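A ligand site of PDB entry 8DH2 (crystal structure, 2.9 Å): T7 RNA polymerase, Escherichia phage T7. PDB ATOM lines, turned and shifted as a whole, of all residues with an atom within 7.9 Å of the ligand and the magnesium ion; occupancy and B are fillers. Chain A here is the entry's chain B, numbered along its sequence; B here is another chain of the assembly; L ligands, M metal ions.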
ATOM      1  N   ASN A 466      18.620 -23.378  17.874  1.00  0.00           N
ATOM      2  CA  ASN A 466      18.615 -22.901  16.501  1.00  0.00           C
ATOM      3  C   ASN A 466      17.320 -22.154  16.161  1.00  0.00           C
ATOM      4  O   ASN A 466      17.333 -21.287  15.278  1.00  0.00           O
ATOM      5  CB  ASN A 466      18.820 -24.065  15.540  1.00  0.00           C
ATOM      6  CG  ASN A 466      20.049 -24.870  15.888  1.00  0.00           C
ATOM      7  OD1 ASN A 466      20.853 -24.482  16.737  1.00  0.00           O
ATOM      8  ND2 ASN A 466      20.217 -26.020  15.237  1.00  0.00           N
ATOM      9  N   ALA A 468      15.971 -20.052  18.154  1.00  0.00           N
ATOM     10  CA  ALA A 468      16.178 -18.731  18.728  1.00  0.00           C
ATOM     11  C   ALA A 468      17.327 -17.975  18.073  1.00  0.00           C
ATOM     12  O   ALA A 468      17.681 -16.882  18.530  1.00  0.00           O
ATOM     13  CB  ALA A 468      16.435 -18.854  20.238  1.00  0.00           C
ATOM     14  N   GLY A 469      17.922 -18.523  17.022  1.00  0.00           N
ATOM     15  CA  GLY A 469      19.050 -17.888  16.365  1.00  0.00           C
ATOM     16  C   GLY A 469      20.385 -18.203  16.977  1.00  0.00           C
ATOM     17  O   GLY A 469      21.401 -17.635  16.534  1.00  0.00           O
ATOM     18  N   VAL A 470      20.440 -19.073  17.977  1.00  0.00           N
ATOM     19  CA  VAL A 470      21.709 -19.423  18.630  1.00  0.00           C
ATOM     20  C   VAL A 470      22.278 -20.610  17.872  1.00  0.00           C
ATOM     21  O   VAL A 470      22.146 -21.773  18.258  1.00  0.00           O
ATOM     22  CB  VAL A 470      21.529 -19.708  20.130  1.00  0.00           C
ATOM     23  CG1 VAL A 470      22.863 -19.707  20.842  1.00  0.00           C
ATOM     24  CG2 VAL A 470      20.603 -18.666  20.745  1.00  0.00           C
ATOM     25  N   ASP A 471      22.949 -20.310  16.746  1.00  0.00           N
ATOM     26  CA  ASP A 471      23.548 -21.335  15.910  1.00  0.00           C
ATOM     27  C   ASP A 471      24.985 -21.026  15.524  1.00  0.00           C
ATOM     28  O   ASP A 471      25.569 -21.744  14.700  1.00  0.00           O
ATOM     29  CB  ASP A 471      22.708 -21.557  14.641  1.00  0.00           C
ATOM     30  CG  ASP A 471      22.229 -20.263  14.031  1.00  0.00           C
ATOM     31  OD1 ASP A 471      22.735 -19.191  14.420  1.00  0.00           O
ATOM     32  OD2 ASP A 471      21.340 -20.311  13.156  1.00  0.00           O
ATOM     33  N   LYS A 472      25.571 -19.966  16.070  1.00  0.00           N
ATOM     34  CA  LYS A 472      26.946 -19.579  15.763  1.00  0.00           C
ATOM     35  C   LYS A 472      27.919 -19.980  16.859  1.00  0.00           C
ATOM     36  O   LYS A 472      29.097 -19.598  16.799  1.00  0.00           O
ATOM     37  CB  LYS A 472      27.014 -18.072  15.503  1.00  0.00           C
ATOM     38  CG  LYS A 472      27.259 -17.716  14.048  1.00  0.00           C
ATOM     39  CD  LYS A 472      26.155 -18.246  13.160  1.00  0.00           C
ATOM     40  CE  LYS A 472      25.054 -17.222  12.975  1.00  0.00           C
ATOM     41  NZ  LYS A 472      24.195 -17.532  11.807  1.00  0.00           N
ATOM     42  N   ASP A 506      14.149 -15.912  16.306  1.00  0.00           N
ATOM     43  CA  ASP A 506      14.347 -15.961  14.860  1.00  0.00           C
ATOM     44  C   ASP A 506      13.275 -16.814  14.187  1.00  0.00           C
ATOM     45  O   ASP A 506      12.787 -16.471  13.096  1.00  0.00           O
ATOM     46  CB  ASP A 506      15.737 -16.504  14.531  1.00  0.00           C
ATOM     47  CG  ASP A 506      16.824 -15.472  14.762  1.00  0.00           C
ATOM     48  OD1 ASP A 506      16.603 -14.535  15.555  1.00  0.00           O
ATOM     49  OD2 ASP A 506      17.902 -15.612  14.149  1.00  0.00           O
ATOM     50  N   GLY A 538      22.431 -27.864   6.339  1.00  0.00           N
ATOM     51  CA  GLY A 538      23.756 -27.593   5.802  1.00  0.00           C
ATOM     52  C   GLY A 538      24.004 -26.098   5.669  1.00  0.00           C
ATOM     53  O   GLY A 538      23.088 -25.322   5.383  1.00  0.00           O
ATOM     54  N   SER A 539      25.258 -25.701   5.910  1.00  0.00           N
ATOM     55  CA  SER A 539      25.590 -24.282   6.073  1.00  0.00           C
ATOM     56  C   SER A 539      25.395 -23.520   4.767  1.00  0.00           C
ATOM     57  O   SER A 539      24.558 -22.615   4.680  1.00  0.00           O
ATOM     58  CB  SER A 539      27.030 -24.152   6.570  1.00  0.00           C
ATOM     59  OG  SER A 539      27.322 -25.117   7.574  1.00  0.00           O
ATOM     60  N   CYS A 540      26.166 -23.875   3.746  1.00  0.00           N
ATOM     61  CA  CYS A 540      25.977 -23.351   2.384  1.00  0.00           C
ATOM     62  C   CYS A 540      26.179 -24.553   1.474  1.00  0.00           C
ATOM     63  O   CYS A 540      27.318 -24.883   1.129  1.00  0.00           O
ATOM     64  CB  CYS A 540      26.943 -22.210   2.061  1.00  0.00           C
ATOM     65  SG  CYS A 540      26.354 -20.553   2.502  1.00  0.00           S
ATOM     66  N   ASP A 569      31.646 -18.970  10.294  1.00  0.00           N
ATOM     67  CA  ASP A 569      30.699 -18.076   9.643  1.00  0.00           C
ATOM     68  C   ASP A 569      31.351 -17.558   8.367  1.00  0.00           C
ATOM     69  O   ASP A 569      32.195 -16.652   8.419  1.00  0.00           O
ATOM     70  CB  ASP A 569      30.310 -16.933  10.587  1.00  0.00           C
ATOM     71  CG  ASP A 569      29.213 -16.058  10.017  1.00  0.00           C
ATOM     72  OD1 ASP A 569      28.489 -16.519   9.118  1.00  0.00           O
ATOM     73  OD2 ASP A 569      29.074 -14.906  10.485  1.00  0.00           O
ATOM     74  N   ILE A 570      30.952 -18.125   7.231  1.00  0.00           N
ATOM     75  CA  ILE A 570      31.587 -17.802   5.953  1.00  0.00           C
ATOM     76  C   ILE A 570      31.355 -16.348   5.570  1.00  0.00           C
ATOM     77  O   ILE A 570      32.163 -15.753   4.839  1.00  0.00           O
ATOM     78  CB  ILE A 570      31.123 -18.783   4.861  1.00  0.00           C
ATOM     79  CG1 ILE A 570      32.061 -18.741   3.653  1.00  0.00           C
ATOM     80  CG2 ILE A 570      29.680 -18.499   4.427  1.00  0.00           C
ATOM     81  CD1 ILE A 570      31.840 -19.853   2.674  1.00  0.00           C
ATOM     82  N   TYR A 571      30.261 -15.739   6.040  1.00  0.00           N
ATOM     83  CA  TYR A 571      30.063 -14.312   5.801  1.00  0.00           C
ATOM     84  C   TYR A 571      31.063 -13.476   6.593  1.00  0.00           C
ATOM     85  O   TYR A 571      31.594 -12.482   6.089  1.00  0.00           O
ATOM     86  CB  TYR A 571      28.630 -13.910   6.149  1.00  0.00           C
ATOM     87  CG  TYR A 571      27.577 -14.887   5.688  1.00  0.00           C
ATOM     88  CD1 TYR A 571      27.536 -15.340   4.370  1.00  0.00           C
ATOM     89  CD2 TYR A 571      26.600 -15.365   6.565  1.00  0.00           C
ATOM     90  CE1 TYR A 571      26.568 -16.243   3.945  1.00  0.00           C
ATOM     91  CE2 TYR A 571      25.638 -16.257   6.157  1.00  0.00           C
ATOM     92  CZ  TYR A 571      25.623 -16.688   4.841  1.00  0.00           C
ATOM     93  OH  TYR A 571      24.661 -17.580   4.432  1.00  0.00           O
ATOM     94  N   GLY A 572      31.330 -13.874   7.836  1.00  0.00           N
ATOM     95  CA  GLY A 572      32.295 -13.151   8.652  1.00  0.00           C
ATOM     96  C   GLY A 572      33.730 -13.457   8.302  1.00  0.00           C
ATOM     97  O   GLY A 572      34.622 -12.646   8.562  1.00  0.00           O
ATOM     98  N   ARG A 627      29.563  -8.941   8.929  1.00  0.00           N
ATOM     99  CA  ARG A 627      29.066 -10.013   8.069  1.00  0.00           C
ATOM    100  C   ARG A 627      27.777  -9.622   7.345  1.00  0.00           C
ATOM    101  O   ARG A 627      27.408 -10.286   6.375  1.00  0.00           O
ATOM    102  CB  ARG A 627      28.837 -11.289   8.866  1.00  0.00           C
ATOM    103  CG  ARG A 627      28.603 -11.073  10.348  1.00  0.00           C
ATOM    104  CD  ARG A 627      27.270 -11.658  10.786  1.00  0.00           C
ATOM    105  NE  ARG A 627      27.193 -13.086  10.527  1.00  0.00           N
ATOM    106  CZ  ARG A 627      26.099 -13.723  10.138  1.00  0.00           C
ATOM    107  NH1 ARG A 627      24.954 -13.080   9.945  1.00  0.00           N
ATOM    108  NH2 ARG A 627      26.140 -15.035   9.928  1.00  0.00           N
ATOM    109  N   SER A 628      27.090  -8.572   7.796  1.00  0.00           N
ATOM    110  CA  SER A 628      25.920  -8.082   7.083  1.00  0.00           C
ATOM    111  C   SER A 628      26.306  -7.437   5.754  1.00  0.00           C
ATOM    112  O   SER A 628      25.493  -7.400   4.825  1.00  0.00           O
ATOM    113  CB  SER A 628      25.150  -7.088   7.942  1.00  0.00           C
ATOM    114  OG  SER A 628      25.217  -7.440   9.313  1.00  0.00           O
ATOM    115  N   LYS A 631      27.122 -10.688   3.307  1.00  0.00           N
ATOM    116  CA  LYS A 631      26.318 -11.905   3.435  1.00  0.00           C
ATOM    117  C   LYS A 631      25.706 -12.305   2.104  1.00  0.00           C
ATOM    118  O   LYS A 631      25.828 -13.468   1.686  1.00  0.00           O
ATOM    119  CB  LYS A 631      25.229 -11.714   4.486  1.00  0.00           C
ATOM    120  CG  LYS A 631      24.457 -12.988   4.802  1.00  0.00           C
ATOM    121  CD  LYS A 631      23.668 -12.855   6.098  1.00  0.00           C
ATOM    122  CE  LYS A 631      22.177 -12.729   5.830  1.00  0.00           C
ATOM    123  NZ  LYS A 631      21.381 -12.890   7.075  1.00  0.00           N
ATOM    124  N   ARG A 632      25.044 -11.370   1.415  1.00  0.00           N
ATOM    125  CA  ARG A 632      24.302 -11.697   0.211  1.00  0.00           C
ATOM    126  C   ARG A 632      25.223 -12.141  -0.920  1.00  0.00           C
ATOM    127  O   ARG A 632      24.838 -12.999  -1.733  1.00  0.00           O
ATOM    128  CB  ARG A 632      23.448 -10.503  -0.221  1.00  0.00           C
ATOM    129  CG  ARG A 632      22.623 -10.717  -1.475  1.00  0.00           C
ATOM    130  CD  ARG A 632      21.216 -11.167  -1.141  1.00  0.00           C
ATOM    131  NE  ARG A 632      20.550 -10.241  -0.232  1.00  0.00           N
ATOM    132  CZ  ARG A 632      19.328  -9.739  -0.432  1.00  0.00           C
ATOM    133  NH1 ARG A 632      18.615 -10.061  -1.500  1.00  0.00           N
ATOM    134  NH2 ARG A 632      18.815  -8.904   0.467  1.00  0.00           N
ATOM    135  N   MET A 635      25.999 -15.710  -0.394  1.00  0.00           N
ATOM    136  CA  MET A 635      24.796 -16.515  -0.591  1.00  0.00           C
ATOM    137  C   MET A 635      24.444 -16.670  -2.061  1.00  0.00           C
ATOM    138  O   MET A 635      23.940 -17.723  -2.476  1.00  0.00           O
ATOM    139  CB  MET A 635      23.627 -15.901   0.168  1.00  0.00           C
ATOM    140  CG  MET A 635      23.621 -16.229   1.644  1.00  0.00           C
ATOM    141  SD  MET A 635      22.161 -15.648   2.537  1.00  0.00           S
ATOM    142  CE  MET A 635      21.323 -14.665   1.301  1.00  0.00           C
ATOM    143  P     A B  11      10.605 -17.912   4.220  1.00  0.00           P
ATOM    144  OP1   A B  11      10.713 -18.220   5.661  1.00  0.00           O
ATOM    145  OP2   A B  11      11.429 -16.818   3.624  1.00  0.00           O
ATOM    146  O5'   A B  11      10.911 -19.248   3.404  1.00  0.00           O
ATOM    147  C5'   A B  11      10.238 -20.460   3.724  1.00  0.00           C
ATOM    148  C4'   A B  11      10.625 -21.573   2.787  1.00  0.00           C
ATOM    149  O4'   A B  11      10.104 -21.312   1.450  1.00  0.00           O
ATOM    150  C3'   A B  11      12.115 -21.766   2.555  1.00  0.00           C
ATOM    151  O3'   A B  11      12.748 -22.467   3.605  1.00  0.00           O
ATOM    152  C2'   A B  11      12.160 -22.484   1.213  1.00  0.00           C
ATOM    153  O2'   A B  11      11.860 -23.866   1.373  1.00  0.00           O
ATOM    154  C1'   A B  11      10.999 -21.822   0.482  1.00  0.00           C
ATOM    155  N9    A B  11      11.454 -20.702  -0.366  1.00  0.00           N
ATOM    156  C8    A B  11      11.295 -19.356  -0.168  1.00  0.00           C
ATOM    157  N7    A B  11      11.830 -18.614  -1.100  1.00  0.00           N
ATOM    158  C5    A B  11      12.388 -19.531  -1.983  1.00  0.00           C
ATOM    159  C6    A B  11      13.091 -19.389  -3.188  1.00  0.00           C
ATOM    160  N6    A B  11      13.384 -18.204  -3.734  1.00  0.00           N
ATOM    161  N1    A B  11      13.519 -20.509  -3.811  1.00  0.00           N
ATOM    162  C2    A B  11      13.236 -21.697  -3.266  1.00  0.00           C
ATOM    163  N3    A B  11      12.564 -21.960  -2.140  1.00  0.00           N
ATOM    164  C4    A B  11      12.169 -20.822  -1.537  1.00  0.00           C
ATOM    165  P     U B  12      14.018 -21.813   4.338  1.00  0.00           P
ATOM    166  OP1   U B  12      14.144 -22.518   5.640  1.00  0.00           O
ATOM    167  OP2   U B  12      13.787 -20.352   4.333  1.00  0.00           O
ATOM    168  O5'   U B  12      15.232 -22.229   3.398  1.00  0.00           O
ATOM    169  C5'   U B  12      15.588 -23.606   3.408  1.00  0.00           C
ATOM    170  C4'   U B  12      16.239 -24.102   2.146  1.00  0.00           C
ATOM    171  O4'   U B  12      15.437 -23.739   0.999  1.00  0.00           O
ATOM    172  C3'   U B  12      17.633 -23.583   1.820  1.00  0.00           C
ATOM    173  C2'   U B  12      17.701 -23.833   0.323  1.00  0.00           C
ATOM    174  O2'   U B  12      17.950 -25.211   0.082  1.00  0.00           O
ATOM    175  C1'   U B  12      16.274 -23.522  -0.122  1.00  0.00           C
ATOM    176  N1    U B  12      16.141 -22.122  -0.596  1.00  0.00           N
ATOM    177  C2    U B  12      16.611 -21.802  -1.860  1.00  0.00           C
ATOM    178  O2    U B  12      17.138 -22.614  -2.619  1.00  0.00           O
ATOM    179  N3    U B  12      16.462 -20.484  -2.227  1.00  0.00           N
ATOM    180  C4    U B  12      15.900 -19.468  -1.482  1.00  0.00           C
ATOM    181  O4    U B  12      15.835 -18.339  -1.959  1.00  0.00           O
ATOM    182  C5    U B  12      15.426 -19.866  -0.190  1.00  0.00           C
ATOM    183  C6    U B  12      15.565 -21.147   0.192  1.00  0.00           C
HETATM  184  P1  LIG L   1      22.642 -16.029   9.245  1.00  0.00           P
HETATM  185  O1  LIG L   1      21.848 -17.083   9.991  1.00  0.00           O
HETATM  186  O2  LIG L   1      22.327 -14.666   9.800  1.00  0.00           O
HETATM  187  O3  LIG L   1      24.118 -16.314   9.387  1.00  0.00           O
HETATM  188  P2  LIG L   1      21.799 -17.456   6.859  1.00  0.00           P
HETATM  189  O4  LIG L   1      22.228 -17.368   5.414  1.00  0.00           O
HETATM  190  O5  LIG L   1      22.458 -18.640   7.527  1.00  0.00           O
HETATM  191  O6  LIG L   1      22.217 -16.075   7.651  1.00  0.00           O
HETATM  192  P3  LIG L   1      19.146 -16.334   7.159  1.00  0.00           P
HETATM  193  O7  LIG L   1      17.754 -16.706   6.696  1.00  0.00           O
HETATM  194  O8  LIG L   1      19.121 -15.970   8.617  1.00  0.00           O
HETATM  195  O9  LIG L   1      20.160 -17.611   6.931  1.00  0.00           O
HETATM  196  O10 LIG L   1      19.642 -15.152   6.356  1.00  0.00           O
HETATM  197 MG    MG M   1      20.032 -17.390  11.192  1.00  0.00          MG
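The magnesium ion is bound by an oxygen (O1) of the ligand (2.2 Å).
The magnesium ion has one donor atom within binding distance.
SD of Met 635 sits close to O4 of the ligand.
Of the 21 residues printed, 5 come within 4 Å of the ligand.
Along chain A the residues within 4 Å of the ligand span positions 472 to 635.
The nearest printed residue that does not touch the ligand is Asp 569 (4.4 Å).
Residues that only touch the magnesium ion: Asp 471 (3.8 Å).
Of the 21 residues printed, 1 comes within 4 Å of the magnesium ion.
The nearest printed residue that does not touch the magnesium ion is Asp 506 (4.1 Å).
OD2 of Asp 569 is in salt-bridge range of NE of Arg 627, at 2.6 Å.
The side-chain hydroxyl (OH) of Tyr 571 sits close to the side-chain sulfur (SD) of Met 635, 3.7 Å away.
The side-chain carboxylate (OD1) of Asp 471 lies within salt-bridge range of the side-chain amino group (NZ) of Lys 472 (3.4 Å).
NH2 of Arg 627 is in salt-bridge range of O3 of the ligand.
An oxygen (O4) of the ligand sits at hydrogen-bond distance from the side-chain hydroxyl (OH) of Tyr 571, 2.6 Å away.
The side-chain amino group of Lys 472 is in salt-bridge range of an oxygen (O3) of the ligand (2.7 Å).
The side-chain amino group (NZ) of Lys 631 lies within salt-bridge range of an oxygen (O10) of the ligand, at 2.9 Å.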
